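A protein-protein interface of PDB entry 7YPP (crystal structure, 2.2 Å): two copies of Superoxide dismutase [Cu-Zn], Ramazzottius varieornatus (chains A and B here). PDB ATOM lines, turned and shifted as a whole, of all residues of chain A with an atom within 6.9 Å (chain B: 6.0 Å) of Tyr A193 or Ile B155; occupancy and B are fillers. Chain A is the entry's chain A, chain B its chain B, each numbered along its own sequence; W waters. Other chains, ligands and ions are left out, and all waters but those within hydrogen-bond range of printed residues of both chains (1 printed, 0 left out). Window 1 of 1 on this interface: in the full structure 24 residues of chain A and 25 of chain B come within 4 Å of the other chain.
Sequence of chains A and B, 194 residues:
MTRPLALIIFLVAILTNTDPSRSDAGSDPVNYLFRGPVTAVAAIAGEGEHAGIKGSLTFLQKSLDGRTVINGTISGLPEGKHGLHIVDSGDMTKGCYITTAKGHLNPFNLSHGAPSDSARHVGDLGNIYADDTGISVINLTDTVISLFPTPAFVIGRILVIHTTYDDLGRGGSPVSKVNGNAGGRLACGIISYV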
ATOM      1  N   TYR A  32     -20.857 -35.656  -1.084  1.00  0.00           N
ATOM      2  CA  TYR A  32     -21.040 -35.218  -2.462  1.00  0.00           C
ATOM      3  C   TYR A  32     -19.721 -34.754  -3.083  1.00  0.00           C
ATOM      4  O   TYR A  32     -19.609 -34.723  -4.315  1.00  0.00           O
ATOM      5  CB  TYR A  32     -22.133 -34.147  -2.574  1.00  0.00           C
ATOM      6  CG  TYR A  32     -21.688 -32.729  -2.310  1.00  0.00           C
ATOM      7  CD1 TYR A  32     -21.578 -32.240  -1.010  1.00  0.00           C
ATOM      8  CD2 TYR A  32     -21.371 -31.872  -3.361  1.00  0.00           C
ATOM      9  CE1 TYR A  32     -21.189 -30.933  -0.755  1.00  0.00           C
ATOM     10  CE2 TYR A  32     -20.956 -30.564  -3.121  1.00  0.00           C
ATOM     11  CZ  TYR A  32     -20.872 -30.095  -1.815  1.00  0.00           C
ATOM     12  OH  TYR A  32     -20.468 -28.806  -1.582  1.00  0.00           O
ATOM     13  N   LEU A  33     -18.733 -34.399  -2.240  1.00  0.00           N
ATOM     14  CA  LEU A  33     -17.445 -33.949  -2.749  1.00  0.00           C
ATOM     15  C   LEU A  33     -16.651 -35.100  -3.356  1.00  0.00           C
ATOM     16  O   LEU A  33     -15.687 -34.846  -4.070  1.00  0.00           O
ATOM     17  CB  LEU A  33     -16.628 -33.309  -1.622  1.00  0.00           C
ATOM     18  CG  LEU A  33     -17.228 -32.057  -0.977  1.00  0.00           C
ATOM     19  CD1 LEU A  33     -16.477 -31.744   0.295  1.00  0.00           C
ATOM     20  CD2 LEU A  33     -17.203 -30.858  -1.924  1.00  0.00           C
ATOM     21  N   VAL A  38     -16.551 -34.080 -11.464  1.00  0.00           N
ATOM     22  CA  VAL A  38     -16.326 -32.780 -10.853  1.00  0.00           C
ATOM     23  C   VAL A  38     -15.781 -31.853 -11.927  1.00  0.00           C
ATOM     24  O   VAL A  38     -14.865 -32.224 -12.650  1.00  0.00           O
ATOM     25  CB  VAL A  38     -15.377 -32.830  -9.632  1.00  0.00           C
ATOM     26  CG1 VAL A  38     -15.066 -31.433  -9.124  1.00  0.00           C
ATOM     27  CG2 VAL A  38     -15.989 -33.621  -8.489  1.00  0.00           C
ATOM     28  N   THR A  39     -16.362 -30.656 -11.997  1.00  0.00           N
ATOM     29  CA  THR A  39     -15.830 -29.594 -12.832  1.00  0.00           C
ATOM     30  C   THR A  39     -15.289 -28.487 -11.928  1.00  0.00           C
ATOM     31  O   THR A  39     -15.968 -28.048 -11.015  1.00  0.00           O
ATOM     32  CB  THR A  39     -16.865 -29.106 -13.861  1.00  0.00           C
ATOM     33  OG1 THR A  39     -17.362 -30.252 -14.561  1.00  0.00           O
ATOM     34  CG2 THR A  39     -16.259 -28.189 -14.894  1.00  0.00           C
ATOM     35  N   ALA A  40     -14.031 -28.095 -12.161  1.00  0.00           N
ATOM     36  CA  ALA A  40     -13.435 -26.950 -11.502  1.00  0.00           C
ATOM     37  C   ALA A  40     -13.011 -25.920 -12.548  1.00  0.00           C
ATOM     38  O   ALA A  40     -12.927 -26.245 -13.733  1.00  0.00           O
ATOM     39  CB  ALA A  40     -12.268 -27.379 -10.667  1.00  0.00           C
ATOM     40  N   VAL A  41     -12.791 -24.674 -12.094  1.00  0.00           N
ATOM     41  CA  VAL A  41     -12.417 -23.586 -12.989  1.00  0.00           C
ATOM     42  C   VAL A  41     -11.388 -22.680 -12.319  1.00  0.00           C
ATOM     43  O   VAL A  41     -11.333 -22.584 -11.104  1.00  0.00           O
ATOM     44  CB  VAL A  41     -13.643 -22.751 -13.436  1.00  0.00           C
ATOM     45  CG1 VAL A  41     -14.534 -23.538 -14.398  1.00  0.00           C
ATOM     46  CG2 VAL A  41     -14.444 -22.227 -12.242  1.00  0.00           C
ATOM     47  N   LEU A 147      -9.520 -33.417  -8.393  1.00  0.00           N
ATOM     48  CA  LEU A 147     -10.606 -32.483  -8.136  1.00  0.00           C
ATOM     49  C   LEU A 147     -11.438 -32.999  -6.971  1.00  0.00           C
ATOM     50  O   LEU A 147     -12.442 -32.381  -6.589  1.00  0.00           O
ATOM     51  CB  LEU A 147     -11.463 -32.329  -9.405  1.00  0.00           C
ATOM     52  CG  LEU A 147     -10.723 -31.787 -10.629  1.00  0.00           C
ATOM     53  CD1 LEU A 147     -11.680 -31.501 -11.785  1.00  0.00           C
ATOM     54  CD2 LEU A 147      -9.855 -30.579 -10.279  1.00  0.00           C
ATOM     55  N   PHE A 148     -11.022 -34.152  -6.425  1.00  0.00           N
ATOM     56  CA  PHE A 148     -11.686 -34.798  -5.296  1.00  0.00           C
ATOM     57  C   PHE A 148     -10.771 -34.632  -4.091  1.00  0.00           C
ATOM     58  O   PHE A 148      -9.556 -34.557  -4.267  1.00  0.00           O
ATOM     59  CB  PHE A 148     -11.927 -36.284  -5.604  1.00  0.00           C
ATOM     60  CG  PHE A 148     -12.846 -36.551  -6.777  1.00  0.00           C
ATOM     61  CD1 PHE A 148     -12.360 -36.590  -8.082  1.00  0.00           C
ATOM     62  CD2 PHE A 148     -14.217 -36.680  -6.597  1.00  0.00           C
ATOM     63  CE1 PHE A 148     -13.214 -36.790  -9.154  1.00  0.00           C
ATOM     64  CE2 PHE A 148     -15.063 -36.916  -7.667  1.00  0.00           C
ATOM     65  CZ  PHE A 148     -14.557 -36.982  -8.946  1.00  0.00           C
ATOM     66  N   PRO A 149     -11.289 -34.527  -2.848  1.00  0.00           N
ATOM     67  CA  PRO A 149     -10.432 -34.232  -1.693  1.00  0.00           C
ATOM     68  C   PRO A 149      -9.541 -35.397  -1.275  1.00  0.00           C
ATOM     69  O   PRO A 149      -9.610 -35.871  -0.148  1.00  0.00           O
ATOM     70  CB  PRO A 149     -11.426 -33.845  -0.581  1.00  0.00           C
ATOM     71  CG  PRO A 149     -12.741 -33.587  -1.324  1.00  0.00           C
ATOM     72  CD  PRO A 149     -12.714 -34.580  -2.475  1.00  0.00           C
ATOM     73  N   PHE A 153      -5.438 -33.149  -4.161  1.00  0.00           N
ATOM     74  CA  PHE A 153      -6.484 -32.146  -4.356  1.00  0.00           C
ATOM     75  C   PHE A 153      -5.851 -30.812  -4.758  1.00  0.00           C
ATOM     76  O   PHE A 153      -4.931 -30.351  -4.080  1.00  0.00           O
ATOM     77  CB  PHE A 153      -7.218 -31.960  -3.031  1.00  0.00           C
ATOM     78  CG  PHE A 153      -8.571 -31.300  -3.044  1.00  0.00           C
ATOM     79  CD1 PHE A 153      -9.483 -31.544  -4.067  1.00  0.00           C
ATOM     80  CD2 PHE A 153      -8.968 -30.485  -1.990  1.00  0.00           C
ATOM     81  CE1 PHE A 153     -10.748 -30.971  -4.052  1.00  0.00           C
ATOM     82  CE2 PHE A 153     -10.226 -29.906  -1.981  1.00  0.00           C
ATOM     83  CZ  PHE A 153     -11.116 -30.178  -2.998  1.00  0.00           C
ATOM     84  N   ILE A 155      -7.941 -27.981  -5.642  1.00  0.00           N
ATOM     85  CA  ILE A 155      -8.915 -26.916  -5.443  1.00  0.00           C
ATOM     86  C   ILE A 155      -8.484 -26.054  -4.248  1.00  0.00           C
ATOM     87  O   ILE A 155      -7.971 -26.572  -3.248  1.00  0.00           O
ATOM     88  CB  ILE A 155     -10.342 -27.506  -5.315  1.00  0.00           C
ATOM     89  CG1 ILE A 155     -10.931 -27.771  -6.705  1.00  0.00           C
ATOM     90  CG2 ILE A 155     -11.258 -26.593  -4.510  1.00  0.00           C
ATOM     91  CD1 ILE A 155     -11.959 -28.863  -6.776  1.00  0.00           C
ATOM     92  N   GLY A 156      -8.658 -24.731  -4.377  1.00  0.00           N
ATOM     93  CA  GLY A 156      -8.316 -23.770  -3.339  1.00  0.00           C
ATOM     94  C   GLY A 156      -6.831 -23.415  -3.353  1.00  0.00           C
ATOM     95  O   GLY A 156      -6.326 -22.860  -2.376  1.00  0.00           O
ATOM     96  N   ARG A 157      -6.148 -23.764  -4.464  1.00  0.00           N
ATOM     97  CA  ARG A 157      -4.756 -23.380  -4.680  1.00  0.00           C
ATOM     98  C   ARG A 157      -4.674 -22.475  -5.921  1.00  0.00           C
ATOM     99  O   ARG A 157      -5.562 -22.513  -6.777  1.00  0.00           O
ATOM    100  CB  ARG A 157      -3.892 -24.631  -4.905  1.00  0.00           C
ATOM    101  CG  ARG A 157      -4.056 -25.726  -3.861  1.00  0.00           C
ATOM    102  CD  ARG A 157      -3.386 -25.468  -2.529  1.00  0.00           C
ATOM    103  NE  ARG A 157      -3.842 -26.474  -1.577  1.00  0.00           N
ATOM    104  CZ  ARG A 157      -3.529 -26.486  -0.277  1.00  0.00           C
ATOM    105  NH1 ARG A 157      -2.744 -25.544   0.235  1.00  0.00           N
ATOM    106  NH2 ARG A 157      -4.033 -27.431   0.504  1.00  0.00           N
ATOM    107  N   ILE A 190      -7.299 -18.741  -8.630  1.00  0.00           N
ATOM    108  CA  ILE A 190      -7.603 -19.843  -7.732  1.00  0.00           C
ATOM    109  C   ILE A 190      -8.421 -20.895  -8.479  1.00  0.00           C
ATOM    110  O   ILE A 190      -9.412 -20.557  -9.130  1.00  0.00           O
ATOM    111  CB  ILE A 190      -8.341 -19.319  -6.487  1.00  0.00           C
ATOM    112  CG1 ILE A 190      -7.514 -18.235  -5.779  1.00  0.00           C
ATOM    113  CG2 ILE A 190      -8.707 -20.462  -5.549  1.00  0.00           C
ATOM    114  CD1 ILE A 190      -8.365 -17.265  -4.948  1.00  0.00           C
ATOM    115  N   ILE A 191      -8.003 -22.161  -8.367  1.00  0.00           N
ATOM    116  CA  ILE A 191      -8.806 -23.272  -8.848  1.00  0.00           C
ATOM    117  C   ILE A 191      -9.984 -23.447  -7.894  1.00  0.00           C
ATOM    118  O   ILE A 191      -9.782 -23.671  -6.714  1.00  0.00           O
ATOM    119  CB  ILE A 191      -7.959 -24.556  -8.989  1.00  0.00           C
ATOM    120  CG1 ILE A 191      -6.730 -24.312  -9.874  1.00  0.00           C
ATOM    121  CG2 ILE A 191      -8.808 -25.699  -9.520  1.00  0.00           C
ATOM    122  CD1 ILE A 191      -5.716 -25.441  -9.867  1.00  0.00           C
ATOM    123  N   SER A 192     -11.211 -23.322  -8.413  1.00  0.00           N
ATOM    124  CA  SER A 192     -12.425 -23.307  -7.606  1.00  0.00           C
ATOM    125  C   SER A 192     -13.443 -24.262  -8.203  1.00  0.00           C
ATOM    126  O   SER A 192     -13.320 -24.628  -9.367  1.00  0.00           O
ATOM    127  CB  SER A 192     -13.013 -21.916  -7.546  1.00  0.00           C
ATOM    128  OG  SER A 192     -11.996 -20.938  -7.489  1.00  0.00           O
ATOM    129  N   TYR A 193     -14.473 -24.581  -7.409  1.00  0.00           N
ATOM    130  CA  TYR A 193     -15.595 -25.374  -7.885  1.00  0.00           C
ATOM    131  C   TYR A 193     -16.447 -24.589  -8.873  1.00  0.00           C
ATOM    132  O   TYR A 193     -16.642 -23.407  -8.668  1.00  0.00           O
ATOM    133  CB  TYR A 193     -16.446 -25.815  -6.689  1.00  0.00           C
ATOM    134  CG  TYR A 193     -15.835 -26.931  -5.880  1.00  0.00           C
ATOM    135  CD1 TYR A 193     -15.759 -28.229  -6.390  1.00  0.00           C
ATOM    136  CD2 TYR A 193     -15.383 -26.699  -4.585  1.00  0.00           C
ATOM    137  CE1 TYR A 193     -15.207 -29.258  -5.652  1.00  0.00           C
ATOM    138  CE2 TYR A 193     -14.847 -27.730  -3.816  1.00  0.00           C
ATOM    139  CZ  TYR A 193     -14.784 -29.009  -4.351  1.00  0.00           C
ATOM    140  OH  TYR A 193     -14.265 -30.015  -3.601  1.00  0.00           O
ATOM    141  N   VAL A 194     -16.968 -25.259  -9.901  1.00  0.00           N
ATOM    142  CA  VAL A 194     -17.908 -24.633 -10.824  1.00  0.00           C
ATOM    143  C   VAL A 194     -19.231 -24.355 -10.096  1.00  0.00           C
ATOM    144  O   VAL A 194     -19.636 -25.086  -9.173  1.00  0.00           O
ATOM    145  CB  VAL A 194     -18.096 -25.457 -12.118  1.00  0.00           C
ATOM    146  CG1 VAL A 194     -19.174 -24.878 -13.017  1.00  0.00           C
ATOM    147  CG2 VAL A 194     -16.786 -25.498 -12.877  1.00  0.00           C
ATOM    148  OXT VAL A 194     -19.932 -23.369 -10.442  1.00  0.00           O
ATOM    149  N   VAL B  38      -6.716 -25.996  10.033  1.00  0.00           N
ATOM    150  CA  VAL B  38      -6.772 -25.561   8.649  1.00  0.00           C
ATOM    151  C   VAL B  38      -7.008 -24.058   8.632  1.00  0.00           C
ATOM    152  O   VAL B  38      -7.869 -23.556   9.346  1.00  0.00           O
ATOM    153  CB  VAL B  38      -7.849 -26.279   7.819  1.00  0.00           C
ATOM    154  CG1 VAL B  38      -7.882 -25.700   6.408  1.00  0.00           C
ATOM    155  CG2 VAL B  38      -7.686 -27.796   7.818  1.00  0.00           C
ATOM    156  N   THR B  39      -6.217 -23.348   7.826  1.00  0.00           N
ATOM    157  CA  THR B  39      -6.368 -21.918   7.650  1.00  0.00           C
ATOM    158  C   THR B  39      -6.784 -21.648   6.204  1.00  0.00           C
ATOM    159  O   THR B  39      -6.189 -22.198   5.261  1.00  0.00           O
ATOM    160  CB  THR B  39      -5.075 -21.183   8.025  1.00  0.00           C
ATOM    161  OG1 THR B  39      -4.658 -21.636   9.313  1.00  0.00           O
ATOM    162  CG2 THR B  39      -5.251 -19.677   8.020  1.00  0.00           C
ATOM    163  N   ALA B  40      -7.828 -20.837   6.033  1.00  0.00           N
ATOM    164  CA  ALA B  40      -8.272 -20.418   4.712  1.00  0.00           C
ATOM    165  C   ALA B  40      -8.351 -18.892   4.687  1.00  0.00           C
ATOM    166  O   ALA B  40      -8.359 -18.247   5.750  1.00  0.00           O
ATOM    167  CB  ALA B  40      -9.607 -21.064   4.378  1.00  0.00           C
ATOM    168  N   ASP B  88     -23.187 -21.693  -3.899  1.00  0.00           N
ATOM    169  CA  ASP B  88     -22.924 -23.084  -4.230  1.00  0.00           C
ATOM    170  C   ASP B  88     -21.852 -23.201  -5.317  1.00  0.00           C
ATOM    171  O   ASP B  88     -21.417 -24.301  -5.654  1.00  0.00           O
ATOM    172  CB  ASP B  88     -24.212 -23.865  -4.504  1.00  0.00           C
ATOM    173  CG  ASP B  88     -24.972 -23.488  -5.766  1.00  0.00           C
ATOM    174  OD1 ASP B  88     -24.488 -22.630  -6.544  1.00  0.00           O
ATOM    175  OD2 ASP B  88     -26.057 -24.056  -5.961  1.00  0.00           O
ATOM    176  N   SER B  89     -21.410 -22.061  -5.843  1.00  0.00           N
ATOM    177  CA  SER B  89     -20.445 -22.043  -6.930  1.00  0.00           C
ATOM    178  C   SER B  89     -19.167 -21.334  -6.480  1.00  0.00           C
ATOM    179  O   SER B  89     -19.200 -20.472  -5.606  1.00  0.00           O
ATOM    180  CB  SER B  89     -21.056 -21.361  -8.132  1.00  0.00           C
ATOM    181  OG  SER B  89     -20.089 -21.077  -9.123  1.00  0.00           O
ATOM    182  N   GLY B  90     -18.048 -21.682  -7.104  1.00  0.00           N
ATOM    183  CA  GLY B  90     -16.803 -20.960  -6.891  1.00  0.00           C
ATOM    184  C   GLY B  90     -16.318 -20.288  -8.166  1.00  0.00           C
ATOM    185  O   GLY B  90     -15.197 -19.789  -8.225  1.00  0.00           O
ATOM    186  N   ASP B  91     -17.194 -20.247  -9.167  1.00  0.00           N
ATOM    187  CA  ASP B  91     -16.828 -19.870 -10.521  1.00  0.00           C
ATOM    188  C   ASP B  91     -16.842 -18.350 -10.660  1.00  0.00           C
ATOM    189  O   ASP B  91     -17.903 -17.730 -10.688  1.00  0.00           O
ATOM    190  CB  ASP B  91     -17.784 -20.528 -11.516  1.00  0.00           C
ATOM    191  CG  ASP B  91     -17.457 -20.268 -12.977  1.00  0.00           C
ATOM    192  OD1 ASP B  91     -16.518 -19.467 -13.262  1.00  0.00           O
ATOM    193  OD2 ASP B  91     -18.139 -20.885 -13.824  1.00  0.00           O
ATOM    194  N   SER B 146     -17.266 -25.816   7.124  1.00  0.00           N
ATOM    195  CA  SER B 146     -16.085 -26.619   7.402  1.00  0.00           C
ATOM    196  C   SER B 146     -14.941 -26.211   6.475  1.00  0.00           C
ATOM    197  O   SER B 146     -15.181 -25.921   5.308  1.00  0.00           O
ATOM    198  CB  SER B 146     -16.404 -28.093   7.291  1.00  0.00           C
ATOM    199  OG  SER B 146     -15.264 -28.869   7.585  1.00  0.00           O
ATOM    200  N   LEU B 147     -13.715 -26.225   7.013  1.00  0.00           N
ATOM    201  CA  LEU B 147     -12.496 -26.029   6.237  1.00  0.00           C
ATOM    202  C   LEU B 147     -11.893 -27.401   5.896  1.00  0.00           C
ATOM    203  O   LEU B 147     -10.848 -27.474   5.263  1.00  0.00           O
ATOM    204  CB  LEU B 147     -11.518 -25.165   7.037  1.00  0.00           C
ATOM    205  CG  LEU B 147     -12.030 -23.767   7.421  1.00  0.00           C
ATOM    206  CD1 LEU B 147     -10.911 -22.906   8.037  1.00  0.00           C
ATOM    207  CD2 LEU B 147     -12.642 -23.050   6.205  1.00  0.00           C
ATOM    208  N   PHE B 148     -12.575 -28.473   6.321  1.00  0.00           N
ATOM    209  CA  PHE B 148     -12.173 -29.848   6.091  1.00  0.00           C
ATOM    210  C   PHE B 148     -13.142 -30.429   5.056  1.00  0.00           C
ATOM    211  O   PHE B 148     -14.301 -30.011   5.004  1.00  0.00           O
ATOM    212  CB  PHE B 148     -12.237 -30.657   7.393  1.00  0.00           C
ATOM    213  CG  PHE B 148     -11.307 -30.214   8.500  1.00  0.00           C
ATOM    214  CD1 PHE B 148     -11.620 -29.171   9.356  1.00  0.00           C
ATOM    215  CD2 PHE B 148     -10.091 -30.856   8.700  1.00  0.00           C
ATOM    216  CE1 PHE B 148     -10.767 -28.802  10.400  1.00  0.00           C
ATOM    217  CE2 PHE B 148      -9.232 -30.469   9.734  1.00  0.00           C
ATOM    218  CZ  PHE B 148      -9.555 -29.416  10.563  1.00  0.00           C
ATOM    219  N   PHE B 153     -17.918 -28.392   3.523  1.00  0.00           N
ATOM    220  CA  PHE B 153     -16.699 -27.771   3.024  1.00  0.00           C
ATOM    221  C   PHE B 153     -17.038 -26.475   2.294  1.00  0.00           C
ATOM    222  O   PHE B 153     -17.879 -26.484   1.402  1.00  0.00           O
ATOM    223  CB  PHE B 153     -16.077 -28.728   2.001  1.00  0.00           C
ATOM    224  CG  PHE B 153     -14.614 -28.560   1.675  1.00  0.00           C
ATOM    225  CD1 PHE B 153     -13.699 -28.171   2.646  1.00  0.00           C
ATOM    226  CD2 PHE B 153     -14.156 -28.848   0.394  1.00  0.00           C
ATOM    227  CE1 PHE B 153     -12.352 -28.076   2.349  1.00  0.00           C
ATOM    228  CE2 PHE B 153     -12.806 -28.732   0.091  1.00  0.00           C
ATOM    229  CZ  PHE B 153     -11.908 -28.357   1.072  1.00  0.00           C
ATOM    230  N   VAL B 154     -16.335 -25.383   2.617  1.00  0.00           N
ATOM    231  CA  VAL B 154     -16.630 -24.099   1.988  1.00  0.00           C
ATOM    232  C   VAL B 154     -15.489 -23.644   1.077  1.00  0.00           C
ATOM    233  O   VAL B 154     -15.657 -22.668   0.368  1.00  0.00           O
ATOM    234  CB  VAL B 154     -17.017 -23.013   3.021  1.00  0.00           C
ATOM    235  CG1 VAL B 154     -18.288 -23.392   3.760  1.00  0.00           C
ATOM    236  CG2 VAL B 154     -15.890 -22.704   4.003  1.00  0.00           C
ATOM    237  N   ILE B 155     -14.361 -24.354   1.085  1.00  0.00           N
ATOM    238  CA  ILE B 155     -13.239 -24.020   0.226  1.00  0.00           C
ATOM    239  C   ILE B 155     -13.603 -24.254  -1.244  1.00  0.00           C
ATOM    240  O   ILE B 155     -14.273 -25.229  -1.569  1.00  0.00           O
ATOM    241  CB  ILE B 155     -11.957 -24.754   0.683  1.00  0.00           C
ATOM    242  CG1 ILE B 155     -11.314 -24.013   1.863  1.00  0.00           C
ATOM    243  CG2 ILE B 155     -10.949 -24.890  -0.454  1.00  0.00           C
ATOM    244  CD1 ILE B 155     -10.598 -24.898   2.828  1.00  0.00           C
ATOM    245  N   GLY B 156     -13.185 -23.313  -2.112  1.00  0.00           N
ATOM    246  CA  GLY B 156     -13.447 -23.362  -3.544  1.00  0.00           C
ATOM    247  C   GLY B 156     -14.844 -22.860  -3.888  1.00  0.00           C
ATOM    248  O   GLY B 156     -15.325 -23.126  -4.989  1.00  0.00           O
ATOM    249  N   ARG B 157     -15.483 -22.167  -2.934  1.00  0.00           N
ATOM    250  CA  ARG B 157     -16.780 -21.538  -3.131  1.00  0.00           C
ATOM    251  C   ARG B 157     -16.637 -20.026  -2.926  1.00  0.00           C
ATOM    252  O   ARG B 157     -15.730 -19.576  -2.241  1.00  0.00           O
ATOM    253  CB  ARG B 157     -17.840 -22.076  -2.154  1.00  0.00           C
ATOM    254  CG  ARG B 157     -17.917 -23.589  -2.064  1.00  0.00           C
ATOM    255  CD  ARG B 157     -18.626 -24.273  -3.198  1.00  0.00           C
ATOM    256  NE  ARG B 157     -18.375 -25.716  -3.100  1.00  0.00           N
ATOM    257  CZ  ARG B 157     -18.776 -26.616  -3.999  1.00  0.00           C
ATOM    258  NH1 ARG B 157     -19.475 -26.244  -5.057  1.00  0.00           N
ATOM    259  NH2 ARG B 157     -18.453 -27.882  -3.838  1.00  0.00           N
ATOM    260  N   ILE B 190     -13.261 -15.956  -3.572  1.00  0.00           N
ATOM    261  CA  ILE B 190     -13.219 -17.397  -3.387  1.00  0.00           C
ATOM    262  C   ILE B 190     -12.528 -17.696  -2.059  1.00  0.00           C
ATOM    263  O   ILE B 190     -11.443 -17.165  -1.773  1.00  0.00           O
ATOM    264  CB  ILE B 190     -12.481 -18.051  -4.573  1.00  0.00           C
ATOM    265  CG1 ILE B 190     -13.136 -17.667  -5.911  1.00  0.00           C
ATOM    266  CG2 ILE B 190     -12.390 -19.565  -4.369  1.00  0.00           C
ATOM    267  CD1 ILE B 190     -12.216 -17.776  -7.115  1.00  0.00           C
ATOM    268  N   ILE B 191     -13.163 -18.549  -1.246  1.00  0.00           N
ATOM    269  CA  ILE B 191     -12.514 -19.073  -0.055  1.00  0.00           C
ATOM    270  C   ILE B 191     -11.465 -20.088  -0.506  1.00  0.00           C
ATOM    271  O   ILE B 191     -11.801 -21.065  -1.177  1.00  0.00           O
ATOM    272  CB  ILE B 191     -13.549 -19.674   0.920  1.00  0.00           C
ATOM    273  CG1 ILE B 191     -14.644 -18.655   1.251  1.00  0.00           C
ATOM    274  CG2 ILE B 191     -12.863 -20.215   2.166  1.00  0.00           C
ATOM    275  CD1 ILE B 191     -15.847 -19.210   1.964  1.00  0.00           C
ATOM    276  N   SER B 192     -10.199 -19.823  -0.151  1.00  0.00           N
ATOM    277  CA  SER B 192      -9.074 -20.615  -0.641  1.00  0.00           C
ATOM    278  C   SER B 192      -8.160 -20.960   0.524  1.00  0.00           C
ATOM    279  O   SER B 192      -8.252 -20.319   1.564  1.00  0.00           O
ATOM    280  CB  SER B 192      -8.296 -19.882  -1.702  1.00  0.00           C
ATOM    281  OG  SER B 192      -8.336 -18.484  -1.455  1.00  0.00           O
ATOM    282  N   TYR B 193      -7.248 -21.919   0.321  1.00  0.00           N
ATOM    283  CA  TYR B 193      -6.282 -22.273   1.354  1.00  0.00           C
ATOM    284  C   TYR B 193      -5.229 -21.177   1.501  1.00  0.00           C
ATOM    285  O   TYR B 193      -4.856 -20.573   0.508  1.00  0.00           O
ATOM    286  CB  TYR B 193      -5.600 -23.594   1.018  1.00  0.00           C
ATOM    287  CG  TYR B 193      -6.468 -24.818   1.167  1.00  0.00           C
ATOM    288  CD1 TYR B 193      -6.802 -25.305   2.421  1.00  0.00           C
ATOM    289  CD2 TYR B 193      -6.888 -25.526   0.051  1.00  0.00           C
ATOM    290  CE1 TYR B 193      -7.547 -26.469   2.563  1.00  0.00           C
ATOM    291  CE2 TYR B 193      -7.639 -26.692   0.175  1.00  0.00           C
ATOM    292  CZ  TYR B 193      -7.971 -27.159   1.434  1.00  0.00           C
ATOM    293  OH  TYR B 193      -8.717 -28.288   1.554  1.00  0.00           O
HETATM  294  O   HOH W   1     -20.210 -28.003   0.753  1.00  0.00           O
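Leu A33 touches Phe B153 (CD1 to CB, 3.5 Å).
Leu A33 touches Arg B157 (CD2 to NH2, 3.8 Å).
Asp B91 touches Val A41 (OD1 to CG2, 3.6 Å).
Tyr B193 touches Ile A155.
CB of Ser B192 touches O of Gly A156 (3.6 Å).
NH2 of Arg A157 touches CD2 of Tyr B193, at 3.5 Å.
CG2 of Ile B190 touches CG2 of Ile A190 (3.97 Å).
Ile A190 touches Ser B192 (CD1 to OG, 3.7 Å).
Ser A192 touches Gly B156.
NH2 of Arg B157 touches CD2 of Tyr A193 (3.4 Å).
OH of Tyr A32 is in hydrogen-bond range of NH2 of Arg B157 (3.2 Å).
The backbone NH (N) of Tyr B193 lies within hydrogen-bond range of the backbone carbonyl oxygen (O) of Gly A156, 3.0 Å away.
The side-chain hydroxyl (OG) of Ser A192 lies close to the backbone carbonyl oxygen (O) of Gly B90, at 3.5 Å.
The backbone NH (N) of Gly B90 sits at hydrogen-bond distance from the backbone carbonyl oxygen (O) of Tyr A193 (2.7 Å).
The backbone carbonyl oxygen (O) of Tyr A193 sits at hydrogen-bond distance from the backbone NH (N) of Asp B91 (3.2 Å).
N of Tyr A193 lies within hydrogen-bond range of O of Gly B156.
The chain-end carboxylate (OXT) of Val A194 sits at hydrogen-bond distance from the side-chain hydroxyl (OG) of Ser B89 (2.6 Å).
The backbone carbonyl oxygen (O) of Thr A39 lies within hydrogen-bond range of the backbone NH (N) of Val A194 (3.2 Å).
O of Ser A192 sits at hydrogen-bond distance from N of Val A41 (2.8 Å).
The backbone NH (N) of Gly A156 is in hydrogen-bond range of the backbone carbonyl oxygen (O) of Ile A191 (2.8 Å).
O of Arg A157 sits at hydrogen-bond distance from N of Ile A191, at 2.9 Å.
The backbone carbonyl oxygen of Ile A190 sits at hydrogen-bond distance from the side-chain hydroxyl of Ser A192 (3.1 Å).
The side-chain hydroxyl (OG) of Ser B192 is in hydrogen-bond range of the backbone carbonyl oxygen (O) of Ile B190 (3.4 Å).
Of the printed residues of chain B, Phe A153 touches Phe B153.
Of the printed residues of chain B, Arg A157 touches Tyr B193 (3.5 Å).
Of chain B, only Ser B89 (3.9 Å), Gly B90 (2.7 Å), Asp B91 (3.2 Å), Ile B155 (3.4 Å), Gly B156 (2.9 Å) and Arg B157 (3.4 Å) come within 4 Å of Tyr A193.
Ala B40 touches none of the printed residues of chain A.
Ser B146 touches none of the printed residues of chain A.
Ile B155 touches one residue of chain A.
The nearest residue of chain B that does not touch Tyr A193 is Phe B153 (4.2 Å).
The nearest residue of chain A that does not touch Ile B155 is Gly A156 (4.1 Å).
Water W1 lies within hydrogen-bond range of the side-chain hydroxyl (OH) of Tyr A32 and the backbone carbonyl oxygen (O) of Phe B153.
Of the 19 printed residues of chain B, 10 touch a printed residue of chain A.
Of the 18 printed residues of chain A, 11 touch a printed residue of chain B.
Among the printed residues, 22 pairs touch across the chains.
Among the printed residues, no Asp or Glu carboxylate lies within 4 Å of a Lys or Arg side-chain nitrogen of the other chain.
Phe B153 touches its own counterpart, Phe A153.
Gly A156 touches Tyr B193, and with the chains exchanged Tyr A193 touches Gly B156.
Arg A157 touches Tyr B193, and with the chains exchanged Tyr A193 touches Arg B157.
Ile B190 touches its own counterpart, Ile A190.
Of the 22 pairs that touch across the chains among the printed residues, 12 have their exchanged pair printed and touching as well.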
